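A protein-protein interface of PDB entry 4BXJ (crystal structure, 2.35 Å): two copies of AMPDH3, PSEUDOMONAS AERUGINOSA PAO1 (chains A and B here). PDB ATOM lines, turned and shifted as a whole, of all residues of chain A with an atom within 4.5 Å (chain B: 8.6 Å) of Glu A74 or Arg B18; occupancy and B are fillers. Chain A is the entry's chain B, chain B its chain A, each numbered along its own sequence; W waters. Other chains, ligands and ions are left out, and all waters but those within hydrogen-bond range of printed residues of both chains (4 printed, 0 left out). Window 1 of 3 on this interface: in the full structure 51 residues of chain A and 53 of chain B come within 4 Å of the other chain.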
ATOM      1  N   VAL A  19      -7.496  10.656 -15.539  1.00  0.00           N
ATOM      2  CA  VAL A  19      -6.733  11.823 -15.131  1.00  0.00           C
ATOM      3  C   VAL A  19      -7.629  13.064 -15.066  1.00  0.00           C
ATOM      4  O   VAL A  19      -8.447  13.294 -15.955  1.00  0.00           O
ATOM      5  CB  VAL A  19      -5.569  12.075 -16.119  1.00  0.00           C
ATOM      6  CG1 VAL A  19      -4.947  13.443 -15.888  1.00  0.00           C
ATOM      7  CG2 VAL A  19      -4.524  10.991 -15.980  1.00  0.00           C
ATOM      8  N   HIS A  46       5.687  12.872 -15.779  1.00  0.00           N
ATOM      9  CA  HIS A  46       5.312  12.661 -17.167  1.00  0.00           C
ATOM     10  C   HIS A  46       6.123  13.537 -18.095  1.00  0.00           C
ATOM     11  O   HIS A  46       6.505  13.117 -19.190  1.00  0.00           O
ATOM     12  CB  HIS A  46       3.822  12.889 -17.351  1.00  0.00           C
ATOM     13  CG  HIS A  46       2.983  11.850 -16.683  1.00  0.00           C
ATOM     14  ND1 HIS A  46       2.414  12.038 -15.441  1.00  0.00           N
ATOM     15  CD2 HIS A  46       2.648  10.593 -17.065  1.00  0.00           C
ATOM     16  CE1 HIS A  46       1.752  10.948 -15.093  1.00  0.00           C
ATOM     17  NE2 HIS A  46       1.876  10.056 -16.061  1.00  0.00           N
ATOM     18  N   ALA A  72       4.458   7.778 -20.273  1.00  0.00           N
ATOM     19  CA  ALA A  72       3.269   8.037 -21.074  1.00  0.00           C
ATOM     20  C   ALA A  72       2.150   8.500 -20.170  1.00  0.00           C
ATOM     21  O   ALA A  72       2.074   8.093 -19.011  1.00  0.00           O
ATOM     22  CB  ALA A  72       2.844   6.806 -21.801  1.00  0.00           C
ATOM     23  N   GLU A  73       1.269   9.333 -20.712  1.00  0.00           N
ATOM     24  CA  GLU A  73       0.239   9.973 -19.918  1.00  0.00           C
ATOM     25  C   GLU A  73      -0.697   8.967 -19.300  1.00  0.00           C
ATOM     26  O   GLU A  73      -1.208   9.178 -18.199  1.00  0.00           O
ATOM     27  CB  GLU A  73      -0.548  10.938 -20.773  1.00  0.00           C
ATOM     28  CG  GLU A  73       0.165  12.237 -20.989  1.00  0.00           C
ATOM     29  CD  GLU A  73      -0.702  13.239 -21.709  1.00  0.00           C
ATOM     30  OE1 GLU A  73      -1.873  12.894 -22.004  1.00  0.00           O
ATOM     31  OE2 GLU A  73      -0.228  14.367 -21.981  1.00  0.00           O
ATOM     32  N   GLU A  74      -0.911   7.864 -20.012  1.00  0.00           N
ATOM     33  CA  GLU A  74      -1.809   6.831 -19.545  1.00  0.00           C
ATOM     34  C   GLU A  74      -1.213   6.028 -18.392  1.00  0.00           C
ATOM     35  O   GLU A  74      -1.928   5.285 -17.738  1.00  0.00           O
ATOM     36  CB  GLU A  74      -2.154   5.899 -20.695  1.00  0.00           C
ATOM     37  CG  GLU A  74      -1.069   4.895 -20.987  1.00  0.00           C
ATOM     38  CD  GLU A  74      -1.151   4.355 -22.404  1.00  0.00           C
ATOM     39  OE1 GLU A  74      -1.865   3.342 -22.623  1.00  0.00           O
ATOM     40  OE2 GLU A  74      -0.497   4.963 -23.290  1.00  0.00           O
ATOM     41  N   ASP A  75       0.091   6.185 -18.149  1.00  0.00           N
ATOM     42  CA  ASP A  75       0.777   5.485 -17.068  1.00  0.00           C
ATOM     43  C   ASP A  75       0.976   6.356 -15.837  1.00  0.00           C
ATOM     44  O   ASP A  75       0.876   7.583 -15.895  1.00  0.00           O
ATOM     45  CB  ASP A  75       2.124   4.952 -17.537  1.00  0.00           C
ATOM     46  CG  ASP A  75       1.986   3.758 -18.456  1.00  0.00           C
ATOM     47  OD1 ASP A  75       0.969   3.045 -18.347  1.00  0.00           O
ATOM     48  OD2 ASP A  75       2.887   3.526 -19.285  1.00  0.00           O
ATOM     49  N   ARG A  76       1.269   5.699 -14.722  1.00  0.00           N
ATOM     50  CA  ARG A  76       1.395   6.347 -13.431  1.00  0.00           C
ATOM     51  C   ARG A  76       2.843   6.713 -13.194  1.00  0.00           C
ATOM     52  O   ARG A  76       3.690   5.822 -13.045  1.00  0.00           O
ATOM     53  CB  ARG A  76       0.945   5.377 -12.345  1.00  0.00           C
ATOM     54  CG  ARG A  76       0.764   5.998 -10.977  1.00  0.00           C
ATOM     55  CD  ARG A  76       0.212   4.966  -9.992  1.00  0.00           C
ATOM     56  NE  ARG A  76       0.045   5.552  -8.666  1.00  0.00           N
ATOM     57  CZ  ARG A  76       0.963   5.497  -7.701  1.00  0.00           C
ATOM     58  NH1 ARG A  76       2.109   4.858  -7.924  1.00  0.00           N
ATOM     59  NH2 ARG A  76       0.737   6.076  -6.518  1.00  0.00           N
ATOM     60  N   ASN A  92      -0.954  10.584  -7.502  1.00  0.00           N
ATOM     61  CA  ASN A  92      -0.215   9.945  -8.580  1.00  0.00           C
ATOM     62  C   ASN A  92      -1.180   9.215  -9.492  1.00  0.00           C
ATOM     63  O   ASN A  92      -1.031   9.221 -10.715  1.00  0.00           O
ATOM     64  CB  ASN A  92       0.785   8.931  -8.033  1.00  0.00           C
ATOM     65  CG  ASN A  92       2.154   9.527  -7.798  1.00  0.00           C
ATOM     66  OD1 ASN A  92       2.531  10.512  -8.433  1.00  0.00           O
ATOM     67  ND2 ASN A  92       2.913   8.925  -6.891  1.00  0.00           N
ATOM     68  N   ASP A  93      -2.186   8.600  -8.879  1.00  0.00           N
ATOM     69  CA  ASP A  93      -3.177   7.824  -9.606  1.00  0.00           C
ATOM     70  C   ASP A  93      -3.914   8.621 -10.669  1.00  0.00           C
ATOM     71  O   ASP A  93      -4.081   8.170 -11.793  1.00  0.00           O
ATOM     72  CB  ASP A  93      -4.207   7.258  -8.633  1.00  0.00           C
ATOM     73  CG  ASP A  93      -3.611   6.268  -7.659  1.00  0.00           C
ATOM     74  OD1 ASP A  93      -2.612   5.587  -7.998  1.00  0.00           O
ATOM     75  OD2 ASP A  93      -4.163   6.167  -6.548  1.00  0.00           O
ATOM     76  N   THR A  94      -4.366   9.809 -10.307  1.00  0.00           N
ATOM     77  CA  THR A  94      -5.245  10.557 -11.179  1.00  0.00           C
ATOM     78  C   THR A  94      -4.651  11.840 -11.781  1.00  0.00           C
ATOM     79  O   THR A  94      -5.397  12.737 -12.196  1.00  0.00           O
ATOM     80  CB  THR A  94      -6.531  10.880 -10.445  1.00  0.00           C
ATOM     81  OG1 THR A  94      -6.226  11.228  -9.090  1.00  0.00           O
ATOM     82  CG2 THR A  94      -7.404   9.667 -10.422  1.00  0.00           C
ATOM     83  N   SER A  95      -3.323  11.916 -11.878  1.00  0.00           N
ATOM     84  CA  SER A  95      -2.687  13.156 -12.333  1.00  0.00           C
ATOM     85  C   SER A  95      -1.570  12.994 -13.354  1.00  0.00           C
ATOM     86  O   SER A  95      -0.920  11.963 -13.438  1.00  0.00           O
ATOM     87  CB  SER A  95      -2.117  13.931 -11.142  1.00  0.00           C
ATOM     88  OG  SER A  95      -1.026  13.218 -10.578  1.00  0.00           O
ATOM     89  N   ILE A  96      -1.326  14.053 -14.108  1.00  0.00           N
ATOM     90  CA  ILE A  96      -0.138  14.131 -14.926  1.00  0.00           C
ATOM     91  C   ILE A  96       0.826  15.099 -14.237  1.00  0.00           C
ATOM     92  O   ILE A  96       0.409  16.157 -13.774  1.00  0.00           O
ATOM     93  CB  ILE A  96      -0.506  14.594 -16.326  1.00  0.00           C
ATOM     94  CG1 ILE A  96      -1.170  13.438 -17.084  1.00  0.00           C
ATOM     95  CG2 ILE A  96       0.716  15.104 -17.072  1.00  0.00           C
ATOM     96  CD1 ILE A  96      -1.870  13.845 -18.360  1.00  0.00           C
ATOM     97  N   TYR B  15       8.054   3.900 -12.106  1.00  0.00           N
ATOM     98  CA  TYR B  15       6.729   4.215 -12.637  1.00  0.00           C
ATOM     99  C   TYR B  15       5.878   2.939 -12.741  1.00  0.00           C
ATOM    100  O   TYR B  15       6.402   1.825 -12.653  1.00  0.00           O
ATOM    101  CB  TYR B  15       6.833   4.883 -14.010  1.00  0.00           C
ATOM    102  CG  TYR B  15       6.727   3.914 -15.166  1.00  0.00           C
ATOM    103  CD1 TYR B  15       7.831   3.208 -15.603  1.00  0.00           C
ATOM    104  CD2 TYR B  15       5.527   3.707 -15.825  1.00  0.00           C
ATOM    105  CE1 TYR B  15       7.753   2.331 -16.670  1.00  0.00           C
ATOM    106  CE2 TYR B  15       5.436   2.825 -16.889  1.00  0.00           C
ATOM    107  CZ  TYR B  15       6.555   2.139 -17.310  1.00  0.00           C
ATOM    108  OH  TYR B  15       6.488   1.254 -18.369  1.00  0.00           O
ATOM    109  N   GLY B  16       4.574   3.109 -12.943  1.00  0.00           N
ATOM    110  CA  GLY B  16       3.667   1.984 -13.040  1.00  0.00           C
ATOM    111  C   GLY B  16       2.438   2.221 -13.899  1.00  0.00           C
ATOM    112  O   GLY B  16       2.450   3.064 -14.803  1.00  0.00           O
ATOM    113  N   LYS B  17       1.380   1.463 -13.615  1.00  0.00           N
ATOM    114  CA  LYS B  17       0.101   1.598 -14.304  1.00  0.00           C
ATOM    115  C   LYS B  17      -0.854   2.347 -13.402  1.00  0.00           C
ATOM    116  O   LYS B  17      -0.712   2.301 -12.173  1.00  0.00           O
ATOM    117  CB  LYS B  17      -0.479   0.214 -14.599  1.00  0.00           C
ATOM    118  CG  LYS B  17       0.446  -0.707 -15.371  1.00  0.00           C
ATOM    119  CD  LYS B  17       0.706  -0.161 -16.745  1.00  0.00           C
ATOM    120  CE  LYS B  17       1.520  -1.135 -17.587  1.00  0.00           C
ATOM    121  NZ  LYS B  17       1.763  -0.572 -18.960  1.00  0.00           N
ATOM    122  N   ARG B  18      -1.836   3.035 -13.971  1.00  0.00           N
ATOM    123  CA  ARG B  18      -2.800   3.699 -13.099  1.00  0.00           C
ATOM    124  C   ARG B  18      -3.790   2.683 -12.522  1.00  0.00           C
ATOM    125  O   ARG B  18      -4.332   2.891 -11.439  1.00  0.00           O
ATOM    126  CB  ARG B  18      -3.497   4.878 -13.800  1.00  0.00           C
ATOM    127  CG  ARG B  18      -2.590   5.605 -14.808  1.00  0.00           C
ATOM    128  CD  ARG B  18      -3.188   6.871 -15.388  1.00  0.00           C
ATOM    129  NE  ARG B  18      -2.902   7.971 -14.485  1.00  0.00           N
ATOM    130  CZ  ARG B  18      -2.104   9.004 -14.739  1.00  0.00           C
ATOM    131  NH1 ARG B  18      -1.505   9.162 -15.913  1.00  0.00           N
ATOM    132  NH2 ARG B  18      -1.930   9.897 -13.789  1.00  0.00           N
ATOM    133  N   VAL B  19      -3.979   1.565 -13.220  1.00  0.00           N
ATOM    134  CA  VAL B  19      -4.912   0.514 -12.794  1.00  0.00           C
ATOM    135  C   VAL B  19      -4.272  -0.638 -12.017  1.00  0.00           C
ATOM    136  O   VAL B  19      -3.301  -1.235 -12.470  1.00  0.00           O
ATOM    137  CB  VAL B  19      -5.612  -0.120 -14.009  1.00  0.00           C
ATOM    138  CG1 VAL B  19      -6.424  -1.332 -13.588  1.00  0.00           C
ATOM    139  CG2 VAL B  19      -6.493   0.898 -14.688  1.00  0.00           C
ATOM    140  N   ARG B  20      -4.847  -0.974 -10.867  1.00  0.00           N
ATOM    141  CA  ARG B  20      -4.359  -2.087 -10.075  1.00  0.00           C
ATOM    142  C   ARG B  20      -5.490  -2.943  -9.481  1.00  0.00           C
ATOM    143  O   ARG B  20      -5.225  -3.871  -8.727  1.00  0.00           O
ATOM    144  CB  ARG B  20      -3.448  -1.574  -8.955  1.00  0.00           C
ATOM    145  CG  ARG B  20      -4.124  -0.628  -7.988  1.00  0.00           C
ATOM    146  CD  ARG B  20      -3.127   0.066  -7.052  1.00  0.00           C
ATOM    147  NE  ARG B  20      -2.220   0.941  -7.789  1.00  0.00           N
ATOM    148  CZ  ARG B  20      -0.899   0.793  -7.824  1.00  0.00           C
ATOM    149  NH1 ARG B  20      -0.331  -0.194  -7.137  1.00  0.00           N
ATOM    150  NH2 ARG B  20      -0.147   1.639  -8.535  1.00  0.00           N
ATOM    151  N   PHE B  21      -6.743  -2.631  -9.811  1.00  0.00           N
ATOM    152  CA  PHE B  21      -7.895  -3.367  -9.279  1.00  0.00           C
ATOM    153  C   PHE B  21      -8.813  -3.874 -10.382  1.00  0.00           C
ATOM    154  O   PHE B  21      -8.965  -3.225 -11.420  1.00  0.00           O
ATOM    155  CB  PHE B  21      -8.729  -2.488  -8.350  1.00  0.00           C
ATOM    156  CG  PHE B  21      -7.968  -1.927  -7.212  1.00  0.00           C
ATOM    157  CD1 PHE B  21      -7.521  -2.745  -6.196  1.00  0.00           C
ATOM    158  CD2 PHE B  21      -7.697  -0.572  -7.151  1.00  0.00           C
ATOM    159  CE1 PHE B  21      -6.813  -2.221  -5.137  1.00  0.00           C
ATOM    160  CE2 PHE B  21      -6.990  -0.041  -6.098  1.00  0.00           C
ATOM    161  CZ  PHE B  21      -6.545  -0.862  -5.089  1.00  0.00           C
ATOM    162  N   GLU B  73      -9.949   0.507 -21.515  1.00  0.00           N
ATOM    163  CA  GLU B  73      -9.344   0.274 -20.214  1.00  0.00           C
ATOM    164  C   GLU B  73      -8.735   1.549 -19.642  1.00  0.00           C
ATOM    165  O   GLU B  73      -8.871   1.839 -18.448  1.00  0.00           O
ATOM    166  CB  GLU B  73      -8.283  -0.837 -20.281  1.00  0.00           C
ATOM    167  CG  GLU B  73      -8.849  -2.242 -20.480  1.00  0.00           C
ATOM    168  CD  GLU B  73      -7.770  -3.318 -20.509  1.00  0.00           C
ATOM    169  OE1 GLU B  73      -6.624  -3.020 -20.107  1.00  0.00           O
ATOM    170  OE2 GLU B  73      -8.059  -4.463 -20.934  1.00  0.00           O
ATOM    171  N   GLU B  74      -8.078   2.319 -20.501  1.00  0.00           N
ATOM    172  CA  GLU B  74      -7.433   3.550 -20.059  1.00  0.00           C
ATOM    173  C   GLU B  74      -8.414   4.605 -19.563  1.00  0.00           C
ATOM    174  O   GLU B  74      -8.032   5.494 -18.799  1.00  0.00           O
ATOM    175  CB  GLU B  74      -6.532   4.129 -21.148  1.00  0.00           C
ATOM    176  CG  GLU B  74      -7.243   4.774 -22.306  1.00  0.00           C
ATOM    177  CD  GLU B  74      -6.241   5.318 -23.317  1.00  0.00           C
ATOM    178  OE1 GLU B  74      -5.065   4.891 -23.254  1.00  0.00           O
ATOM    179  OE2 GLU B  74      -6.610   6.171 -24.162  1.00  0.00           O
ATOM    180  N   ASP B  75      -9.678   4.503 -19.966  1.00  0.00           N
ATOM    181  CA  ASP B  75     -10.668   5.462 -19.478  1.00  0.00           C
ATOM    182  C   ASP B  75     -11.316   5.057 -18.159  1.00  0.00           C
ATOM    183  O   ASP B  75     -11.056   3.977 -17.628  1.00  0.00           O
ATOM    184  CB  ASP B  75     -11.732   5.730 -20.525  1.00  0.00           C
ATOM    185  CG  ASP B  75     -11.205   6.545 -21.684  1.00  0.00           C
ATOM    186  OD1 ASP B  75     -10.270   7.347 -21.482  1.00  0.00           O
ATOM    187  OD2 ASP B  75     -11.734   6.387 -22.796  1.00  0.00           O
ATOM    188  N   ARG B  88      -6.905   2.385  -0.715  1.00  0.00           N
ATOM    189  CA  ARG B  88      -7.327   3.354  -1.711  1.00  0.00           C
ATOM    190  C   ARG B  88      -8.836   3.544  -1.632  1.00  0.00           C
ATOM    191  O   ARG B  88      -9.514   2.809  -0.916  1.00  0.00           O
ATOM    192  CB  ARG B  88      -6.876   2.946  -3.110  1.00  0.00           C
ATOM    193  CG  ARG B  88      -5.468   3.447  -3.465  1.00  0.00           C
ATOM    194  CD  ARG B  88      -5.044   2.962  -4.836  1.00  0.00           C
ATOM    195  NE  ARG B  88      -3.849   3.626  -5.352  1.00  0.00           N
ATOM    196  CZ  ARG B  88      -2.616   3.176  -5.175  1.00  0.00           C
ATOM    197  NH1 ARG B  88      -2.417   2.079  -4.471  1.00  0.00           N
ATOM    198  NH2 ARG B  88      -1.588   3.828  -5.691  1.00  0.00           N
ATOM    199  N   LEU B  91     -12.602   3.781  -6.291  1.00  0.00           N
ATOM    200  CA  LEU B  91     -11.954   2.749  -7.096  1.00  0.00           C
ATOM    201  C   LEU B  91     -12.195   2.855  -8.591  1.00  0.00           C
ATOM    202  O   LEU B  91     -11.525   2.175  -9.368  1.00  0.00           O
ATOM    203  CB  LEU B  91     -12.325   1.352  -6.620  1.00  0.00           C
ATOM    204  CG  LEU B  91     -11.754   0.904  -5.276  1.00  0.00           C
ATOM    205  CD1 LEU B  91     -11.361  -0.562  -5.361  1.00  0.00           C
ATOM    206  CD2 LEU B  91     -10.574   1.761  -4.855  1.00  0.00           C
ATOM    207  N   ASN B  92     -13.129   3.713  -8.999  1.00  0.00           N
ATOM    208  CA  ASN B  92     -13.312   3.977 -10.412  1.00  0.00           C
ATOM    209  C   ASN B  92     -12.048   4.514 -11.042  1.00  0.00           C
ATOM    210  O   ASN B  92     -11.798   4.299 -12.225  1.00  0.00           O
ATOM    211  CB  ASN B  92     -14.426   4.980 -10.637  1.00  0.00           C
ATOM    212  CG  ASN B  92     -15.762   4.342 -10.665  1.00  0.00           C
ATOM    213  OD1 ASN B  92     -15.874   3.157 -10.962  1.00  0.00           O
ATOM    214  ND2 ASN B  92     -16.799   5.113 -10.381  1.00  0.00           N
ATOM    215  N   ASP B  93     -11.249   5.222 -10.257  1.00  0.00           N
ATOM    216  CA  ASP B  93     -10.064   5.855 -10.809  1.00  0.00           C
ATOM    217  C   ASP B  93      -9.028   4.810 -11.238  1.00  0.00           C
ATOM    218  O   ASP B  93      -8.365   4.959 -12.260  1.00  0.00           O
ATOM    219  CB  ASP B  93      -9.456   6.817  -9.795  1.00  0.00           C
ATOM    220  CG  ASP B  93     -10.385   7.968  -9.444  1.00  0.00           C
ATOM    221  OD1 ASP B  93     -11.285   8.295 -10.257  1.00  0.00           O
ATOM    222  OD2 ASP B  93     -10.196   8.553  -8.348  1.00  0.00           O
ATOM    223  N   THR B  94      -8.926   3.740 -10.463  1.00  0.00           N
ATOM    224  CA  THR B  94      -7.807   2.823 -10.561  1.00  0.00           C
ATOM    225  C   THR B  94      -8.218   1.374 -10.806  1.00  0.00           C
ATOM    226  O   THR B  94      -7.407   0.467 -10.634  1.00  0.00           O
ATOM    227  CB  THR B  94      -6.999   2.854  -9.268  1.00  0.00           C
ATOM    228  OG1 THR B  94      -7.898   2.733  -8.160  1.00  0.00           O
ATOM    229  CG2 THR B  94      -6.217   4.148  -9.149  1.00  0.00           C
ATOM    230  N   SER B  95      -9.474   1.153 -11.188  1.00  0.00           N
ATOM    231  CA  SER B  95      -9.933  -0.201 -11.481  1.00  0.00           C
ATOM    232  C   SER B  95     -10.496  -0.357 -12.882  1.00  0.00           C
ATOM    233  O   SER B  95     -10.753   0.620 -13.589  1.00  0.00           O
ATOM    234  CB  SER B  95     -11.014  -0.631 -10.493  1.00  0.00           C
ATOM    235  OG  SER B  95     -12.227   0.026 -10.802  1.00  0.00           O
ATOM    236  N   ILE B  96     -10.680  -1.615 -13.262  1.00  0.00           N
ATOM    237  CA  ILE B  96     -11.367  -1.982 -14.478  1.00  0.00           C
ATOM    238  C   ILE B  96     -12.642  -2.702 -14.035  1.00  0.00           C
ATOM    239  O   ILE B  96     -12.609  -3.490 -13.097  1.00  0.00           O
ATOM    240  CB  ILE B  96     -10.475  -2.886 -15.318  1.00  0.00           C
ATOM    241  CG1 ILE B  96      -9.497  -2.038 -16.131  1.00  0.00           C
ATOM    242  CG2 ILE B  96     -11.309  -3.771 -16.241  1.00  0.00           C
ATOM    243  CD1 ILE B  96      -8.441  -2.856 -16.859  1.00  0.00           C
ATOM    244  N   ARG B 134      -1.357  -7.765 -17.775  1.00  0.00           N
ATOM    245  CA  ARG B 134      -0.911  -6.483 -18.327  1.00  0.00           C
ATOM    246  C   ARG B 134      -0.904  -5.431 -17.239  1.00  0.00           C
ATOM    247  O   ARG B 134      -0.551  -4.284 -17.481  1.00  0.00           O
ATOM    248  CB  ARG B 134      -1.774  -6.046 -19.529  1.00  0.00           C
ATOM    249  CG  ARG B 134      -1.648  -6.954 -20.754  1.00  0.00           C
ATOM    250  CD  ARG B 134      -2.517  -6.516 -21.933  1.00  0.00           C
ATOM    251  NE  ARG B 134      -3.933  -6.774 -21.699  1.00  0.00           N
ATOM    252  CZ  ARG B 134      -4.803  -5.860 -21.273  1.00  0.00           C
ATOM    253  NH1 ARG B 134      -4.406  -4.608 -21.050  1.00  0.00           N
ATOM    254  NH2 ARG B 134      -6.068  -6.188 -21.075  1.00  0.00           N
ATOM    255  N   TYR B 135      -1.274  -5.848 -16.034  1.00  0.00           N
ATOM    256  CA  TYR B 135      -1.290  -4.961 -14.885  1.00  0.00           C
ATOM    257  C   TYR B 135      -0.570  -5.575 -13.693  1.00  0.00           C
ATOM    258  O   TYR B 135      -1.209  -6.145 -12.802  1.00  0.00           O
ATOM    259  CB  TYR B 135      -2.733  -4.600 -14.517  1.00  0.00           C
ATOM    260  CG  TYR B 135      -3.396  -3.780 -15.586  1.00  0.00           C
ATOM    261  CD1 TYR B 135      -3.182  -2.410 -15.666  1.00  0.00           C
ATOM    262  CD2 TYR B 135      -4.208  -4.376 -16.538  1.00  0.00           C
ATOM    263  CE1 TYR B 135      -3.770  -1.655 -16.657  1.00  0.00           C
ATOM    264  CE2 TYR B 135      -4.797  -3.635 -17.535  1.00  0.00           C
ATOM    265  CZ  TYR B 135      -4.582  -2.268 -17.589  1.00  0.00           C
ATOM    266  OH  TYR B 135      -5.177  -1.516 -18.576  1.00  0.00           O
ATOM    267  N   PRO B 136       0.767  -5.437 -13.662  1.00  0.00           N
ATOM    268  CA  PRO B 136       1.669  -6.016 -12.656  1.00  0.00           C
ATOM    269  C   PRO B 136       1.256  -5.823 -11.206  1.00  0.00           C
ATOM    270  O   PRO B 136       1.501  -6.734 -10.424  1.00  0.00           O
ATOM    271  CB  PRO B 136       2.992  -5.294 -12.924  1.00  0.00           C
ATOM    272  CG  PRO B 136       2.959  -5.069 -14.391  1.00  0.00           C
ATOM    273  CD  PRO B 136       1.519  -4.722 -14.710  1.00  0.00           C
ATOM    274  N   ASP B 137       0.675  -4.680 -10.842  1.00  0.00           N
ATOM    275  CA  ASP B 137       0.285  -4.447  -9.448  1.00  0.00           C
ATOM    276  C   ASP B 137      -1.137  -4.918  -9.174  1.00  0.00           C
ATOM    277  O   ASP B 137      -1.668  -4.712  -8.072  1.00  0.00           O
ATOM    278  CB  ASP B 137       0.420  -2.970  -9.054  1.00  0.00           C
ATOM    279  CG  ASP B 137       1.853  -2.450  -9.168  1.00  0.00           C
ATOM    280  OD1 ASP B 137       2.794  -3.153  -8.712  1.00  0.00           O
ATOM    281  OD2 ASP B 137       2.027  -1.330  -9.713  1.00  0.00           O
ATOM    282  N   MET B 138      -1.761  -5.535 -10.180  1.00  0.00           N
ATOM    283  CA  MET B 138      -3.063  -6.168  -9.985  1.00  0.00           C
ATOM    284  C   MET B 138      -2.867  -7.577  -9.413  1.00  0.00           C
ATOM    285  O   MET B 138      -3.090  -8.588 -10.080  1.00  0.00           O
ATOM    286  CB  MET B 138      -3.863  -6.194 -11.284  1.00  0.00           C
ATOM    287  CG  MET B 138      -5.295  -6.627 -11.109  1.00  0.00           C
ATOM    288  SD  MET B 138      -6.152  -6.653 -12.686  1.00  0.00           S
ATOM    289  CE  MET B 138      -6.434  -4.899 -12.955  1.00  0.00           C
HETATM  290  O   HOH W   1      -2.756   3.186  -9.108  1.00  0.00           O
HETATM  291  O   HOH W   2      -0.199   1.434 -20.359  1.00  0.00           O
HETATM  292  O   HOH W   3      -5.035   5.848 -18.099  1.00  0.00           O
HETATM  293  O   HOH W   4       2.677   2.275  -9.645  1.00  0.00           O
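Of the 12 printed residues of chain A, 10 touch a printed residue of chain B.
Hydrophobic or aromatic side chains of chain B within 4 Å of the printed part of chain A: Tyr B15.
Among the printed residues, 22 pairs touch across the chains.
Among the printed residues, Asp or Glu carboxylates within 4 Å of a Lys or Arg side-chain nitrogen of the other chain: Asp A75 with Lys B17 (3.8 Å) and Asp A93 with Arg B88 (2.8 Å).
Among the printed residues, pairs that only touch across the chains: Glu A74 with Arg B18 (3.0 Å), Asp A75 with Gly B16 (3.3 Å), Val A19 with Arg B18 (3.4 Å), Arg A76 with Tyr B15 (3.4 Å), Arg A76 with Lys B17 (3.5 Å), His A46 with Arg B18 (3.5 Å), Thr A94 with Asp B93 (3.6 Å), Asp A75 with Tyr B15 (3.6 Å), Glu A74 with Glu B74 (3.6 Å), Arg A76 with Arg B20 (3.6 Å), Asp A93 with Thr B94 (3.7 Å), Arg A76 with Arg B18 (3.9 Å) and Thr A94 with Arg B18 (3.9 Å).
The guanidinium group (NH1) of Arg B20 is in salt-bridge range of the side-chain carboxylate (OD2) of Asp B137, at 3.7 Å.
O of Asp A75 sits at hydrogen-bond distance from NE2 of His A46 (2.7 Å).
The backbone NH (N) of Phe B21 is in hydrogen-bond range of the backbone carbonyl oxygen (O) of Thr B94 (3.3 Å).
The backbone carbonyl oxygen (O) of Thr B94 sits at hydrogen-bond distance from the backbone NH (N) of Arg B20 (2.9 Å).
NE of Arg A76 lies within salt-bridge range of OD1 of Asp A93, 2.7 Å away.
Water W1 lies within hydrogen-bond range of OD1 of Asp A93 (2.6 Å), NE of Arg B20 (2.7 Å) and O of Arg B18 (2.8 Å).
Water W2 lies within hydrogen-bond range of the side-chain carboxylate (OD1) of Asp A75 (2.8 Å), the side-chain amino group (NZ) of Lys B17 (3.1 Å) and the side-chain carboxylate (OE1) of Glu A74 (3.4 Å).
Water W3 bridges O of Glu B74 and O of Glu A74.
Water W4 lies within hydrogen-bond range of the guanidinium group of Arg B20 (3.1 Å) and the guanidinium group of Arg A76 (3.2 Å).
Glu B74 touches its own counterpart, Glu A74.
Asp A93 touches Thr B94, and with the chains exchanged Thr A94 touches Asp B93.
Of the 22 pairs that touch across the chains among the printed residues, 3 have their exchanged pair printed and touching as well.
Of chain B, only Arg B18 (3.0 Å) and Glu B74 (3.6 Å) come within 4 Å of Glu A74.
Of chain B, only Tyr B15, Gly B16, Lys B17 and Arg B18 come within 4 Å of Asp A75.
Of the printed residues of chain B, Ser A95 touches Arg B18.
Of the printed residues of chain A, Lys B17 touches Asp A75 and Arg A76.
Of chain A, only Val A19, His A46, Glu A73, Glu A74, Asp A75, Arg A76, Asn A92, Asp A93, Thr A94 and Ser A95 come within 4 Å of Arg B18.
Val B19 touches none of the printed residues of chain A.
Printed residues of chain A within 4 Å of Arg B20: Arg A76 (3.6 Å).
Printed residues of chain A within 4 Å of Thr B94: Asp A93 (3.7 Å).
The nearest residue of chain B that does not touch Glu A74 is Lys B17 (5.3 Å).
The side-chain amino group (NZ) of Lys B17 is in salt-bridge range of the side-chain carboxylate (OD1) of Asp A75, 3.8 Å away.
NE of Arg B18 is in hydrogen-bond range of O of Asp A93 (2.9 Å).
The backbone carbonyl oxygen of Ser A95 sits close to the guanidinium group of Arg B18 (2.3 Å).
NH1 of Arg B18 lies within hydrogen-bond range of O of Asp A75 (2.9 Å).
The backbone NH (N) of Gly B16 sits at hydrogen-bond distance from the backbone carbonyl oxygen (O) of Arg A76, 2.9 Å away.
NH1 of Arg B18 sits close to O of Glu A73.
The guanidinium group (NH2) of Arg A76 lies close to the guanidinium group (NH2) of Arg B88, 3.3 Å away.
The guanidinium group (NE) of Arg B88 lies within salt-bridge range of the side-chain carboxylate (OD2) of Asp A93 (2.8 Å).
O of Asn A92 lies within hydrogen-bond range of NH2 of Arg B18 (3.3 Å).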
